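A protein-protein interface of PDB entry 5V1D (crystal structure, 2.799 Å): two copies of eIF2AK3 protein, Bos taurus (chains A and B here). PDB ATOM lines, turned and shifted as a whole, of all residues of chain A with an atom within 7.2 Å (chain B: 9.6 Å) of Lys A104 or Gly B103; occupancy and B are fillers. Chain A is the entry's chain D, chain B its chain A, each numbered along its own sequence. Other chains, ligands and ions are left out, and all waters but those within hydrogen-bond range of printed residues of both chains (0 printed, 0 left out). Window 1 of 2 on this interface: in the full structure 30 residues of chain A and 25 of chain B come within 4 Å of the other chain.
The backbone carbonyl oxygen (O) of Leu B106 sits at hydrogen-bond distance from the backbone NH (N) of Gly A102 (2.9 Å).
The backbone carbonyl oxygen (O) of Lys B104 lies within hydrogen-bond range of the backbone NH (N) of Lys A104, 2.7 Å away.
The guanidinium group (NE) of Arg B152 sits at hydrogen-bond distance from the backbone carbonyl oxygen (O) of Ala A124, at 3.2 Å.
The guanidinium group (NH2) of Arg B152 is in hydrogen-bond range of the backbone carbonyl oxygen (O) of Leu A125, at 3.4 Å.
The backbone carbonyl oxygen (O) of Gly B102 is in hydrogen-bond range of the backbone NH (N) of Leu A106.
N of Val B101 is in hydrogen-bond range of O of Arg B152, 2.6 Å away.
The backbone carbonyl oxygen of Thr B150 lies within hydrogen-bond range of the backbone NH of Gly B103 (3.1 Å).
The side-chain amino group of Lys A104 is in salt-bridge range of the side-chain carboxylate of Glu A85 (2.9 Å).
The backbone NH (N) of Leu A125 sits close to the side-chain hydroxyl (OG) of Ser A123.
N of Gly A103 is in hydrogen-bond range of O of Thr A150, 3.1 Å away.
The side-chain amino group of Lys B104 is in salt-bridge range of the side-chain carboxylate of Glu B85 (2.9 Å).
Among the printed residues, pairs that only touch across the chains: Leu A88 with Leu B106 (3.6 Å), Gly A102 with Ala B124 (3.9 Å), Gly A103 with Lys B104 (3.1 Å), Lys A104 with Gly B103 (3.2 Å), Leu A106 with Leu B100 (3.2 Å), Leu A106 with Val B101 (3.7 Å), Ser A123 with Val B101 (3.8 Å), Ser A123 with Arg B152 (3.7 Å), Ala A124 with Gly B102 (3.5 Å), Ala A124 with Gly B103 (3.6 Å), Ala A124 with Thr B150 (3.4 Å) and Thr A150 with Ala B124 (3.6 Å).
Of chain B, only Lys B104 comes within 4 Å of Gly A103.
Of chain B, only Gly B103 and Lys B104 come within 4 Å of Lys A104.
Of the printed residues of chain A, Leu B100 touches Leu A106.
Of the printed residues of chain A, Leu B106 touches Leu A88 and Gly A102.
Of the printed residues of chain A, Thr B150 touches Ala A124.
Of the 26 printed residues of chain B, 9 touch a printed residue of chain A.
Printed residues of chain A that touch a printed residue of chain B: Leu A88, Gly A102, Gly A103, Lys A104, Leu A106, Ser A123, Ala A124, Leu A125 and Thr A150.
Among the printed residues, 17 pairs touch across the chains.
Among the printed residues, no Asp or Glu carboxylate lies within 4 Å of a Lys or Arg side-chain nitrogen of the other chain.
Leu A88 touches Leu B106, but with the chains exchanged Leu A106 does not touch Leu B88 (4.3 Å).
Gly A102 touches Ala B124, and with the chains exchanged Ala A124 touches Gly B102.
Gly A103 touches Lys B104, and with the chains exchanged Lys A104 touches Gly B103.
Ala A124 touches Thr B150, and with the chains exchanged Thr A150 touches Ala B124.
Of the 17 pairs that touch across the chains among the printed residues, 9 have their exchanged pair printed and touching as well.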
ATOM      1  N   GLU A  85      -5.889 -24.290 -32.607  1.00  0.00           N
ATOM      2  CA  GLU A  85      -4.835 -23.320 -32.347  1.00  0.00           C
ATOM      3  C   GLU A  85      -5.370 -21.899 -32.285  1.00  0.00           C
ATOM      4  O   GLU A  85      -4.811 -21.064 -31.565  1.00  0.00           O
ATOM      5  CB  GLU A  85      -3.744 -23.426 -33.408  1.00  0.00           C
ATOM      6  CG  GLU A  85      -2.365 -23.603 -32.809  1.00  0.00           C
ATOM      7  CD  GLU A  85      -1.280 -23.660 -33.853  1.00  0.00           C
ATOM      8  OE1 GLU A  85      -1.561 -24.142 -34.969  1.00  0.00           O
ATOM      9  OE2 GLU A  85      -0.150 -23.214 -33.559  1.00  0.00           O
ATOM     10  N   LEU A  88      -6.006 -20.382 -29.163  1.00  0.00           N
ATOM     11  CA  LEU A  88      -4.807 -20.037 -28.414  1.00  0.00           C
ATOM     12  C   LEU A  88      -4.177 -18.738 -28.892  1.00  0.00           C
ATOM     13  O   LEU A  88      -3.041 -18.431 -28.512  1.00  0.00           O
ATOM     14  CB  LEU A  88      -3.798 -21.175 -28.500  1.00  0.00           C
ATOM     15  CG  LEU A  88      -4.396 -22.541 -28.171  1.00  0.00           C
ATOM     16  CD1 LEU A  88      -3.313 -23.618 -28.208  1.00  0.00           C
ATOM     17  CD2 LEU A  88      -5.096 -22.519 -26.821  1.00  0.00           C
ATOM     18  N   GLY A 102      -4.457 -23.904 -21.734  1.00  0.00           N
ATOM     19  CA  GLY A 102      -3.953 -25.019 -22.509  1.00  0.00           C
ATOM     20  C   GLY A 102      -2.509 -24.854 -22.928  1.00  0.00           C
ATOM     21  O   GLY A 102      -1.660 -24.470 -22.119  1.00  0.00           O
ATOM     22  N   GLY A 103      -2.219 -25.146 -24.182  1.00  0.00           N
ATOM     23  CA  GLY A 103      -0.880 -24.996 -24.714  1.00  0.00           C
ATOM     24  C   GLY A 103      -0.616 -25.956 -25.855  1.00  0.00           C
ATOM     25  O   GLY A 103      -1.277 -26.980 -26.026  1.00  0.00           O
ATOM     26  N   LYS A 104       0.386 -25.611 -26.657  1.00  0.00           N
ATOM     27  CA  LYS A 104       0.834 -26.428 -27.773  1.00  0.00           C
ATOM     28  C   LYS A 104       2.185 -27.046 -27.436  1.00  0.00           C
ATOM     29  O   LYS A 104       2.988 -26.459 -26.702  1.00  0.00           O
ATOM     30  CB  LYS A 104       0.939 -25.596 -29.051  1.00  0.00           C
ATOM     31  CG  LYS A 104       1.254 -26.392 -30.298  1.00  0.00           C
ATOM     32  CD  LYS A 104       1.375 -25.469 -31.499  1.00  0.00           C
ATOM     33  CE  LYS A 104       1.626 -26.253 -32.779  1.00  0.00           C
ATOM     34  NZ  LYS A 104       1.763 -25.372 -33.979  1.00  0.00           N
ATOM     35  N   SER A 105       2.429 -28.238 -27.980  1.00  0.00           N
ATOM     36  CA  SER A 105       3.594 -29.032 -27.623  1.00  0.00           C
ATOM     37  C   SER A 105       4.127 -29.785 -28.830  1.00  0.00           C
ATOM     38  O   SER A 105       3.356 -30.339 -29.617  1.00  0.00           O
ATOM     39  CB  SER A 105       3.258 -30.036 -26.516  1.00  0.00           C
ATOM     40  OG  SER A 105       4.204 -31.089 -26.503  1.00  0.00           O
ATOM     41  N   LEU A 106       5.454 -29.811 -28.956  1.00  0.00           N
ATOM     42  CA  LEU A 106       6.145 -30.625 -29.953  1.00  0.00           C
ATOM     43  C   LEU A 106       7.368 -31.247 -29.296  1.00  0.00           C
ATOM     44  O   LEU A 106       8.363 -30.558 -29.052  1.00  0.00           O
ATOM     45  CB  LEU A 106       6.555 -29.805 -31.174  1.00  0.00           C
ATOM     46  CG  LEU A 106       7.339 -30.627 -32.196  1.00  0.00           C
ATOM     47  CD1 LEU A 106       6.700 -30.536 -33.569  1.00  0.00           C
ATOM     48  CD2 LEU A 106       8.784 -30.181 -32.251  1.00  0.00           C
ATOM     49  N   SER A 123      12.187 -32.421 -25.216  1.00  0.00           N
ATOM     50  CA  SER A 123      10.928 -31.711 -25.083  1.00  0.00           C
ATOM     51  C   SER A 123      11.193 -30.216 -24.981  1.00  0.00           C
ATOM     52  O   SER A 123      12.337 -29.756 -25.009  1.00  0.00           O
ATOM     53  CB  SER A 123      10.161 -32.217 -23.860  1.00  0.00           C
ATOM     54  OG  SER A 123      10.985 -32.191 -22.707  1.00  0.00           O
ATOM     55  N   ALA A 124      10.115 -29.447 -24.858  1.00  0.00           N
ATOM     56  CA  ALA A 124      10.280 -28.036 -24.551  1.00  0.00           C
ATOM     57  C   ALA A 124      10.813 -27.829 -23.142  1.00  0.00           C
ATOM     58  O   ALA A 124      11.287 -26.734 -22.825  1.00  0.00           O
ATOM     59  CB  ALA A 124       8.954 -27.297 -24.719  1.00  0.00           C
ATOM     60  N   LEU A 125      10.757 -28.863 -22.302  1.00  0.00           N
ATOM     61  CA  LEU A 125      11.150 -28.773 -20.904  1.00  0.00           C
ATOM     62  C   LEU A 125      12.626 -29.082 -20.696  1.00  0.00           C
ATOM     63  O   LEU A 125      13.283 -28.436 -19.872  1.00  0.00           O
ATOM     64  CB  LEU A 125      10.305 -29.727 -20.055  1.00  0.00           C
ATOM     65  CG  LEU A 125       8.798 -29.478 -19.927  1.00  0.00           C
ATOM     66  CD1 LEU A 125       8.019 -29.929 -21.163  1.00  0.00           C
ATOM     67  CD2 LEU A 125       8.262 -30.165 -18.682  1.00  0.00           C
ATOM     68  N   THR A 147       3.380 -34.044 -32.020  1.00  0.00           N
ATOM     69  CA  THR A 147       2.694 -32.794 -31.764  1.00  0.00           C
ATOM     70  C   THR A 147       1.469 -33.060 -30.906  1.00  0.00           C
ATOM     71  O   THR A 147       0.775 -34.060 -31.091  1.00  0.00           O
ATOM     72  CB  THR A 147       2.276 -32.132 -33.073  1.00  0.00           C
ATOM     73  OG1 THR A 147       3.415 -32.049 -33.936  1.00  0.00           O
ATOM     74  CG2 THR A 147       1.734 -30.742 -32.811  1.00  0.00           C
ATOM     75  N   GLN A 148       1.218 -32.168 -29.954  1.00  0.00           N
ATOM     76  CA  GLN A 148       0.055 -32.295 -29.087  1.00  0.00           C
ATOM     77  C   GLN A 148      -0.432 -30.901 -28.748  1.00  0.00           C
ATOM     78  O   GLN A 148       0.334 -30.096 -28.212  1.00  0.00           O
ATOM     79  CB  GLN A 148       0.386 -33.069 -27.813  1.00  0.00           C
ATOM     80  CG  GLN A 148      -0.831 -33.406 -26.974  1.00  0.00           C
ATOM     81  CD  GLN A 148      -1.674 -34.522 -27.581  1.00  0.00           C
ATOM     82  OE1 GLN A 148      -1.290 -35.140 -28.577  1.00  0.00           O
ATOM     83  NE2 GLN A 148      -2.826 -34.792 -26.973  1.00  0.00           N
ATOM     84  N   LYS A 149      -1.694 -30.623 -29.061  1.00  0.00           N
ATOM     85  CA  LYS A 149      -2.316 -29.340 -28.771  1.00  0.00           C
ATOM     86  C   LYS A 149      -3.568 -29.579 -27.945  1.00  0.00           C
ATOM     87  O   LYS A 149      -4.515 -30.216 -28.418  1.00  0.00           O
ATOM     88  CB  LYS A 149      -2.661 -28.592 -30.059  1.00  0.00           C
ATOM     89  CG  LYS A 149      -1.562 -28.603 -31.103  1.00  0.00           C
ATOM     90  CD  LYS A 149      -1.787 -27.509 -32.127  1.00  0.00           C
ATOM     91  CE  LYS A 149      -1.801 -28.058 -33.544  1.00  0.00           C
ATOM     92  NZ  LYS A 149      -2.033 -26.967 -34.546  1.00  0.00           N
ATOM     93  N   THR A 150      -3.572 -29.069 -26.721  1.00  0.00           N
ATOM     94  CA  THR A 150      -4.716 -29.168 -25.832  1.00  0.00           C
ATOM     95  C   THR A 150      -5.280 -27.777 -25.566  1.00  0.00           C
ATOM     96  O   THR A 150      -4.543 -26.789 -25.514  1.00  0.00           O
ATOM     97  CB  THR A 150      -4.323 -29.843 -24.515  1.00  0.00           C
ATOM     98  OG1 THR A 150      -5.339 -29.625 -23.531  1.00  0.00           O
ATOM     99  CG2 THR A 150      -3.008 -29.288 -24.014  1.00  0.00           C
ATOM    100  N   VAL B  84       8.788 -17.274 -33.340  1.00  0.00           N
ATOM    101  CA  VAL B  84       9.169 -18.384 -32.466  1.00  0.00           C
ATOM    102  C   VAL B  84       8.459 -19.666 -32.882  1.00  0.00           C
ATOM    103  O   VAL B  84       9.037 -20.758 -32.839  1.00  0.00           O
ATOM    104  CB  VAL B  84       8.891 -18.026 -30.993  1.00  0.00           C
ATOM    105  CG1 VAL B  84       8.777 -19.277 -30.146  1.00  0.00           C
ATOM    106  CG2 VAL B  84      10.001 -17.144 -30.459  1.00  0.00           C
ATOM    107  N   GLU B  85       7.213 -19.554 -33.331  1.00  0.00           N
ATOM    108  CA  GLU B  85       6.483 -20.739 -33.762  1.00  0.00           C
ATOM    109  C   GLU B  85       6.704 -21.061 -35.230  1.00  0.00           C
ATOM    110  O   GLU B  85       6.586 -22.227 -35.621  1.00  0.00           O
ATOM    111  CB  GLU B  85       4.985 -20.572 -33.492  1.00  0.00           C
ATOM    112  CG  GLU B  85       4.660 -20.061 -32.093  1.00  0.00           C
ATOM    113  CD  GLU B  85       3.307 -20.539 -31.591  1.00  0.00           C
ATOM    114  OE1 GLU B  85       3.272 -21.250 -30.564  1.00  0.00           O
ATOM    115  OE2 GLU B  85       2.282 -20.212 -32.223  1.00  0.00           O
ATOM    116  N   SER B  86       7.028 -20.061 -36.051  1.00  0.00           N
ATOM    117  CA  SER B  86       7.299 -20.335 -37.454  1.00  0.00           C
ATOM    118  C   SER B  86       8.514 -21.230 -37.631  1.00  0.00           C
ATOM    119  O   SER B  86       8.630 -21.902 -38.659  1.00  0.00           O
ATOM    120  CB  SER B  86       7.496 -19.031 -38.222  1.00  0.00           C
ATOM    121  OG  SER B  86       6.285 -18.303 -38.291  1.00  0.00           O
ATOM    122  N   LEU B  87       9.413 -21.258 -36.648  1.00  0.00           N
ATOM    123  CA  LEU B  87      10.574 -22.134 -36.734  1.00  0.00           C
ATOM    124  C   LEU B  87      10.206 -23.582 -36.450  1.00  0.00           C
ATOM    125  O   LEU B  87      10.671 -24.490 -37.147  1.00  0.00           O
ATOM    126  CB  LEU B  87      11.654 -21.671 -35.759  1.00  0.00           C
ATOM    127  CG  LEU B  87      12.556 -20.534 -36.224  1.00  0.00           C
ATOM    128  CD1 LEU B  87      13.219 -19.897 -35.026  1.00  0.00           C
ATOM    129  CD2 LEU B  87      13.600 -21.052 -37.199  1.00  0.00           C
ATOM    130  N   LEU B  88       9.374 -23.811 -35.431  1.00  0.00           N
ATOM    131  CA  LEU B  88       9.005 -25.170 -35.060  1.00  0.00           C
ATOM    132  C   LEU B  88       8.290 -25.884 -36.197  1.00  0.00           C
ATOM    133  O   LEU B  88       8.529 -27.071 -36.442  1.00  0.00           O
ATOM    134  CB  LEU B  88       8.128 -25.141 -33.813  1.00  0.00           C
ATOM    135  CG  LEU B  88       8.834 -24.699 -32.535  1.00  0.00           C
ATOM    136  CD1 LEU B  88       7.996 -23.683 -31.797  1.00  0.00           C
ATOM    137  CD2 LEU B  88       9.081 -25.907 -31.663  1.00  0.00           C
ATOM    138  N   GLU B  89       7.418 -25.178 -36.909  1.00  0.00           N
ATOM    139  CA  GLU B  89       6.679 -25.759 -38.023  1.00  0.00           C
ATOM    140  C   GLU B  89       7.574 -25.935 -39.249  1.00  0.00           C
ATOM    141  O   GLU B  89       8.540 -26.702 -39.222  1.00  0.00           O
ATOM    142  CB  GLU B  89       5.463 -24.884 -38.360  1.00  0.00           C
ATOM    143  CG  GLU B  89       4.925 -25.022 -39.782  1.00  0.00           C
ATOM    144  CD  GLU B  89       5.505 -23.983 -40.734  1.00  0.00           C
ATOM    145  OE1 GLU B  89       6.166 -24.374 -41.722  1.00  0.00           O
ATOM    146  OE2 GLU B  89       5.306 -22.775 -40.486  1.00  0.00           O
ATOM    147  N   LEU B 100      14.238 -28.814 -34.134  1.00  0.00           N
ATOM    148  CA  LEU B 100      13.614 -27.869 -33.225  1.00  0.00           C
ATOM    149  C   LEU B 100      12.601 -28.577 -32.336  1.00  0.00           C
ATOM    150  O   LEU B 100      11.870 -29.460 -32.787  1.00  0.00           O
ATOM    151  CB  LEU B 100      12.925 -26.738 -33.990  1.00  0.00           C
ATOM    152  CG  LEU B 100      13.771 -25.842 -34.898  1.00  0.00           C
ATOM    153  CD1 LEU B 100      15.126 -25.542 -34.272  1.00  0.00           C
ATOM    154  CD2 LEU B 100      13.922 -26.436 -36.300  1.00  0.00           C
ATOM    155  N   VAL B 101      12.574 -28.183 -31.066  1.00  0.00           N
ATOM    156  CA  VAL B 101      11.518 -28.577 -30.146  1.00  0.00           C
ATOM    157  C   VAL B 101      11.134 -27.364 -29.320  1.00  0.00           C
ATOM    158  O   VAL B 101      11.917 -26.430 -29.146  1.00  0.00           O
ATOM    159  CB  VAL B 101      11.933 -29.732 -29.224  1.00  0.00           C
ATOM    160  CG1 VAL B 101      11.867 -31.030 -29.977  1.00  0.00           C
ATOM    161  CG2 VAL B 101      13.323 -29.487 -28.698  1.00  0.00           C
ATOM    162  N   GLY B 102       9.913 -27.386 -28.811  1.00  0.00           N
ATOM    163  CA  GLY B 102       9.399 -26.261 -28.056  1.00  0.00           C
ATOM    164  C   GLY B 102       7.890 -26.234 -28.086  1.00  0.00           C
ATOM    165  O   GLY B 102       7.240 -26.948 -28.851  1.00  0.00           O
ATOM    166  N   GLY B 103       7.333 -25.379 -27.232  1.00  0.00           N
ATOM    167  CA  GLY B 103       5.892 -25.293 -27.108  1.00  0.00           C
ATOM    168  C   GLY B 103       5.458 -24.023 -26.417  1.00  0.00           C
ATOM    169  O   GLY B 103       6.154 -23.500 -25.541  1.00  0.00           O
ATOM    170  N   LYS B 104       4.287 -23.534 -26.811  1.00  0.00           N
ATOM    171  CA  LYS B 104       3.651 -22.370 -26.211  1.00  0.00           C
ATOM    172  C   LYS B 104       2.655 -22.825 -25.154  1.00  0.00           C
ATOM    173  O   LYS B 104       1.959 -23.826 -25.341  1.00  0.00           O
ATOM    174  CB  LYS B 104       2.945 -21.534 -27.283  1.00  0.00           C
ATOM    175  CG  LYS B 104       1.824 -20.646 -26.778  1.00  0.00           C
ATOM    176  CD  LYS B 104       0.931 -20.216 -27.924  1.00  0.00           C
ATOM    177  CE  LYS B 104       1.621 -19.196 -28.789  1.00  0.00           C
ATOM    178  NZ  LYS B 104       0.887 -18.961 -30.056  1.00  0.00           N
ATOM    179  N   SER B 105       2.594 -22.091 -24.045  1.00  0.00           N
ATOM    180  CA  SER B 105       1.743 -22.436 -22.915  1.00  0.00           C
ATOM    181  C   SER B 105       0.851 -21.255 -22.570  1.00  0.00           C
ATOM    182  O   SER B 105       1.332 -20.124 -22.457  1.00  0.00           O
ATOM    183  CB  SER B 105       2.580 -22.822 -21.699  1.00  0.00           C
ATOM    184  OG  SER B 105       3.717 -23.570 -22.087  1.00  0.00           O
ATOM    185  N   LEU B 106      -0.439 -21.523 -22.390  1.00  0.00           N
ATOM    186  CA  LEU B 106      -1.422 -20.516 -21.998  1.00  0.00           C
ATOM    187  C   LEU B 106      -1.985 -20.924 -20.645  1.00  0.00           C
ATOM    188  O   LEU B 106      -2.823 -21.827 -20.557  1.00  0.00           O
ATOM    189  CB  LEU B 106      -2.531 -20.384 -23.032  1.00  0.00           C
ATOM    190  CG  LEU B 106      -2.202 -19.640 -24.324  1.00  0.00           C
ATOM    191  CD1 LEU B 106      -1.389 -20.520 -25.257  1.00  0.00           C
ATOM    192  CD2 LEU B 106      -3.474 -19.164 -25.003  1.00  0.00           C
ATOM    193  N   THR B 107      -1.526 -20.253 -19.597  1.00  0.00           N
ATOM    194  CA  THR B 107      -1.960 -20.516 -18.237  1.00  0.00           C
ATOM    195  C   THR B 107      -2.661 -19.284 -17.690  1.00  0.00           C
ATOM    196  O   THR B 107      -2.195 -18.160 -17.884  1.00  0.00           O
ATOM    197  CB  THR B 107      -0.772 -20.878 -17.351  1.00  0.00           C
ATOM    198  OG1 THR B 107       0.034 -21.855 -18.015  1.00  0.00           O
ATOM    199  CG2 THR B 107      -1.250 -21.442 -16.028  1.00  0.00           C
ATOM    200  N   ALA B 124      -3.086 -26.609 -19.033  1.00  0.00           N
ATOM    201  CA  ALA B 124      -3.186 -27.956 -19.572  1.00  0.00           C
ATOM    202  C   ALA B 124      -2.984 -29.002 -18.485  1.00  0.00           C
ATOM    203  O   ALA B 124      -3.576 -30.086 -18.555  1.00  0.00           O
ATOM    204  CB  ALA B 124      -2.176 -28.145 -20.700  1.00  0.00           C
ATOM    205  N   ARG B 146      -0.552 -16.035 -18.776  1.00  0.00           N
ATOM    206  CA  ARG B 146       0.857 -16.054 -19.157  1.00  0.00           C
ATOM    207  C   ARG B 146       1.085 -16.960 -20.364  1.00  0.00           C
ATOM    208  O   ARG B 146       0.703 -18.133 -20.345  1.00  0.00           O
ATOM    209  CB  ARG B 146       1.736 -16.528 -17.997  1.00  0.00           C
ATOM    210  CG  ARG B 146       3.197 -16.209 -18.188  1.00  0.00           C
ATOM    211  CD  ARG B 146       4.105 -17.264 -17.588  1.00  0.00           C
ATOM    212  NE  ARG B 146       5.462 -17.144 -18.119  1.00  0.00           N
ATOM    213  CZ  ARG B 146       6.460 -16.504 -17.513  1.00  0.00           C
ATOM    214  NH1 ARG B 146       6.272 -15.924 -16.334  1.00  0.00           N
ATOM    215  NH2 ARG B 146       7.656 -16.450 -18.085  1.00  0.00           N
ATOM    216  N   THR B 147       1.724 -16.416 -21.400  1.00  0.00           N
ATOM    217  CA  THR B 147       2.099 -17.161 -22.597  1.00  0.00           C
ATOM    218  C   THR B 147       3.621 -17.245 -22.626  1.00  0.00           C
ATOM    219  O   THR B 147       4.300 -16.253 -22.913  1.00  0.00           O
ATOM    220  CB  THR B 147       1.556 -16.497 -23.857  1.00  0.00           C
ATOM    221  OG1 THR B 147       0.127 -16.551 -23.848  1.00  0.00           O
ATOM    222  CG2 THR B 147       2.075 -17.200 -25.090  1.00  0.00           C
ATOM    223  N   GLN B 148       4.150 -18.427 -22.317  1.00  0.00           N
ATOM    224  CA  GLN B 148       5.589 -18.673 -22.318  1.00  0.00           C
ATOM    225  C   GLN B 148       5.935 -19.456 -23.577  1.00  0.00           C
ATOM    226  O   GLN B 148       5.549 -20.619 -23.719  1.00  0.00           O
ATOM    227  CB  GLN B 148       6.025 -19.430 -21.065  1.00  0.00           C
ATOM    228  CG  GLN B 148       7.526 -19.668 -20.976  1.00  0.00           C
ATOM    229  CD  GLN B 148       8.293 -18.455 -20.470  1.00  0.00           C
ATOM    230  OE1 GLN B 148       7.721 -17.383 -20.276  1.00  0.00           O
ATOM    231  NE2 GLN B 148       9.592 -18.623 -20.247  1.00  0.00           N
ATOM    232  N   LYS B 149       6.653 -18.810 -24.486  1.00  0.00           N
ATOM    233  CA  LYS B 149       7.049 -19.406 -25.754  1.00  0.00           C
ATOM    234  C   LYS B 149       8.492 -19.870 -25.638  1.00  0.00           C
ATOM    235  O   LYS B 149       9.408 -19.048 -25.542  1.00  0.00           O
ATOM    236  CB  LYS B 149       6.906 -18.408 -26.900  1.00  0.00           C
ATOM    237  CG  LYS B 149       5.492 -17.990 -27.242  1.00  0.00           C
ATOM    238  CD  LYS B 149       5.532 -16.922 -28.322  1.00  0.00           C
ATOM    239  CE  LYS B 149       4.311 -16.970 -29.217  1.00  0.00           C
ATOM    240  NZ  LYS B 149       4.451 -16.069 -30.401  1.00  0.00           N
ATOM    241  N   THR B 150       8.699 -21.177 -25.656  1.00  0.00           N
ATOM    242  CA  THR B 150      10.036 -21.740 -25.646  1.00  0.00           C
ATOM    243  C   THR B 150      10.271 -22.502 -26.940  1.00  0.00           C
ATOM    244  O   THR B 150       9.333 -23.029 -27.546  1.00  0.00           O
ATOM    245  CB  THR B 150      10.235 -22.666 -24.455  1.00  0.00           C
ATOM    246  OG1 THR B 150       9.755 -23.971 -24.790  1.00  0.00           O
ATOM    247  CG2 THR B 150       9.450 -22.153 -23.263  1.00  0.00           C
ATOM    248  N   VAL B 151      11.527 -22.542 -27.370  1.00  0.00           N
ATOM    249  CA  VAL B 151      11.924 -23.335 -28.527  1.00  0.00           C
ATOM    250  C   VAL B 151      13.376 -23.745 -28.339  1.00  0.00           C
ATOM    251  O   VAL B 151      14.215 -22.923 -27.962  1.00  0.00           O
ATOM    252  CB  VAL B 151      11.723 -22.575 -29.856  1.00  0.00           C
ATOM    253  CG1 VAL B 151      12.420 -21.223 -29.823  1.00  0.00           C
ATOM    254  CG2 VAL B 151      12.219 -23.408 -31.023  1.00  0.00           C
ATOM    255  N   ARG B 152      13.670 -25.020 -28.575  1.00  0.00           N
ATOM    256  CA  ARG B 152      15.008 -25.563 -28.392  1.00  0.00           C
ATOM    257  C   ARG B 152      15.500 -26.168 -29.697  1.00  0.00           C
ATOM    258  O   ARG B 152      14.812 -26.998 -30.302  1.00  0.00           O
ATOM    259  CB  ARG B 152      15.039 -26.624 -27.283  1.00  0.00           C
ATOM    260  CG  ARG B 152      14.666 -26.104 -25.905  1.00  0.00           C
ATOM    261  CD  ARG B 152      14.920 -27.150 -24.828  1.00  0.00           C
ATOM    262  NE  ARG B 152      14.403 -26.733 -23.524  1.00  0.00           N
ATOM    263  CZ  ARG B 152      15.113 -26.094 -22.597  1.00  0.00           C
ATOM    264  NH1 ARG B 152      16.387 -25.788 -22.815  1.00  0.00           N
ATOM    265  NH2 ARG B 152      14.548 -25.761 -21.446  1.00  0.00           N
ATOM    266  N   PHE B 165      15.461 -20.343 -27.018  1.00  0.00           N
ATOM    267  CA  PHE B 165      14.863 -19.077 -26.623  1.00  0.00           C
ATOM    268  C   PHE B 165      13.558 -19.372 -25.906  1.00  0.00           C
ATOM    269  O   PHE B 165      12.767 -20.196 -26.372  1.00  0.00           O
ATOM    270  CB  PHE B 165      14.607 -18.181 -27.838  1.00  0.00           C
ATOM    271  CG  PHE B 165      15.841 -17.876 -28.635  1.00  0.00           C
ATOM    272  CD1 PHE B 165      15.834 -17.989 -30.016  1.00  0.00           C
ATOM    273  CD2 PHE B 165      17.007 -17.467 -28.007  1.00  0.00           C
ATOM    274  CE1 PHE B 165      16.971 -17.707 -30.755  1.00  0.00           C
ATOM    275  CE2 PHE B 165      18.147 -17.185 -28.738  1.00  0.00           C
ATOM    276  CZ  PHE B 165      18.128 -17.305 -30.116  1.00  0.00           C
ATOM    277  N   SER B 166      13.334 -18.708 -24.774  1.00  0.00           N
ATOM    278  CA  SER B 166      12.113 -18.905 -23.991  1.00  0.00           C
ATOM    279  C   SER B 166      11.593 -17.536 -23.560  1.00  0.00           C
ATOM    280  O   SER B 166      12.004 -17.007 -22.526  1.00  0.00           O
ATOM    281  CB  SER B 166      12.368 -19.807 -22.795  1.00  0.00           C
ATOM    282  OG  SER B 166      11.249 -19.811 -21.930  1.00  0.00           O
ATOM    283  N   VAL B 167      10.679 -16.980 -24.351  1.00  0.00           N
ATOM    284  CA  VAL B 167      10.093 -15.680 -24.069  1.00  0.00           C
ATOM    285  C   VAL B 167       8.763 -15.881 -23.360  1.00  0.00           C
ATOM    286  O   VAL B 167       8.139 -16.944 -23.429  1.00  0.00           O
ATOM    287  CB  VAL B 167       9.902 -14.842 -25.348  1.00  0.00           C
ATOM    288  CG1 VAL B 167      11.196 -14.733 -26.107  1.00  0.00           C
ATOM    289  CG2 VAL B 167       8.828 -15.448 -26.217  1.00  0.00           C
ATOM    290  N   GLY B 168       8.311 -14.835 -22.673  1.00  0.00           N
ATOM    291  CA  GLY B 168       7.036 -14.877 -21.990  1.00  0.00           C
ATOM    292  C   GLY B 168       6.324 -13.544 -22.097  1.00  0.00           C
ATOM    293  O   GLY B 168       6.946 -12.494 -22.277  1.00  0.00           O
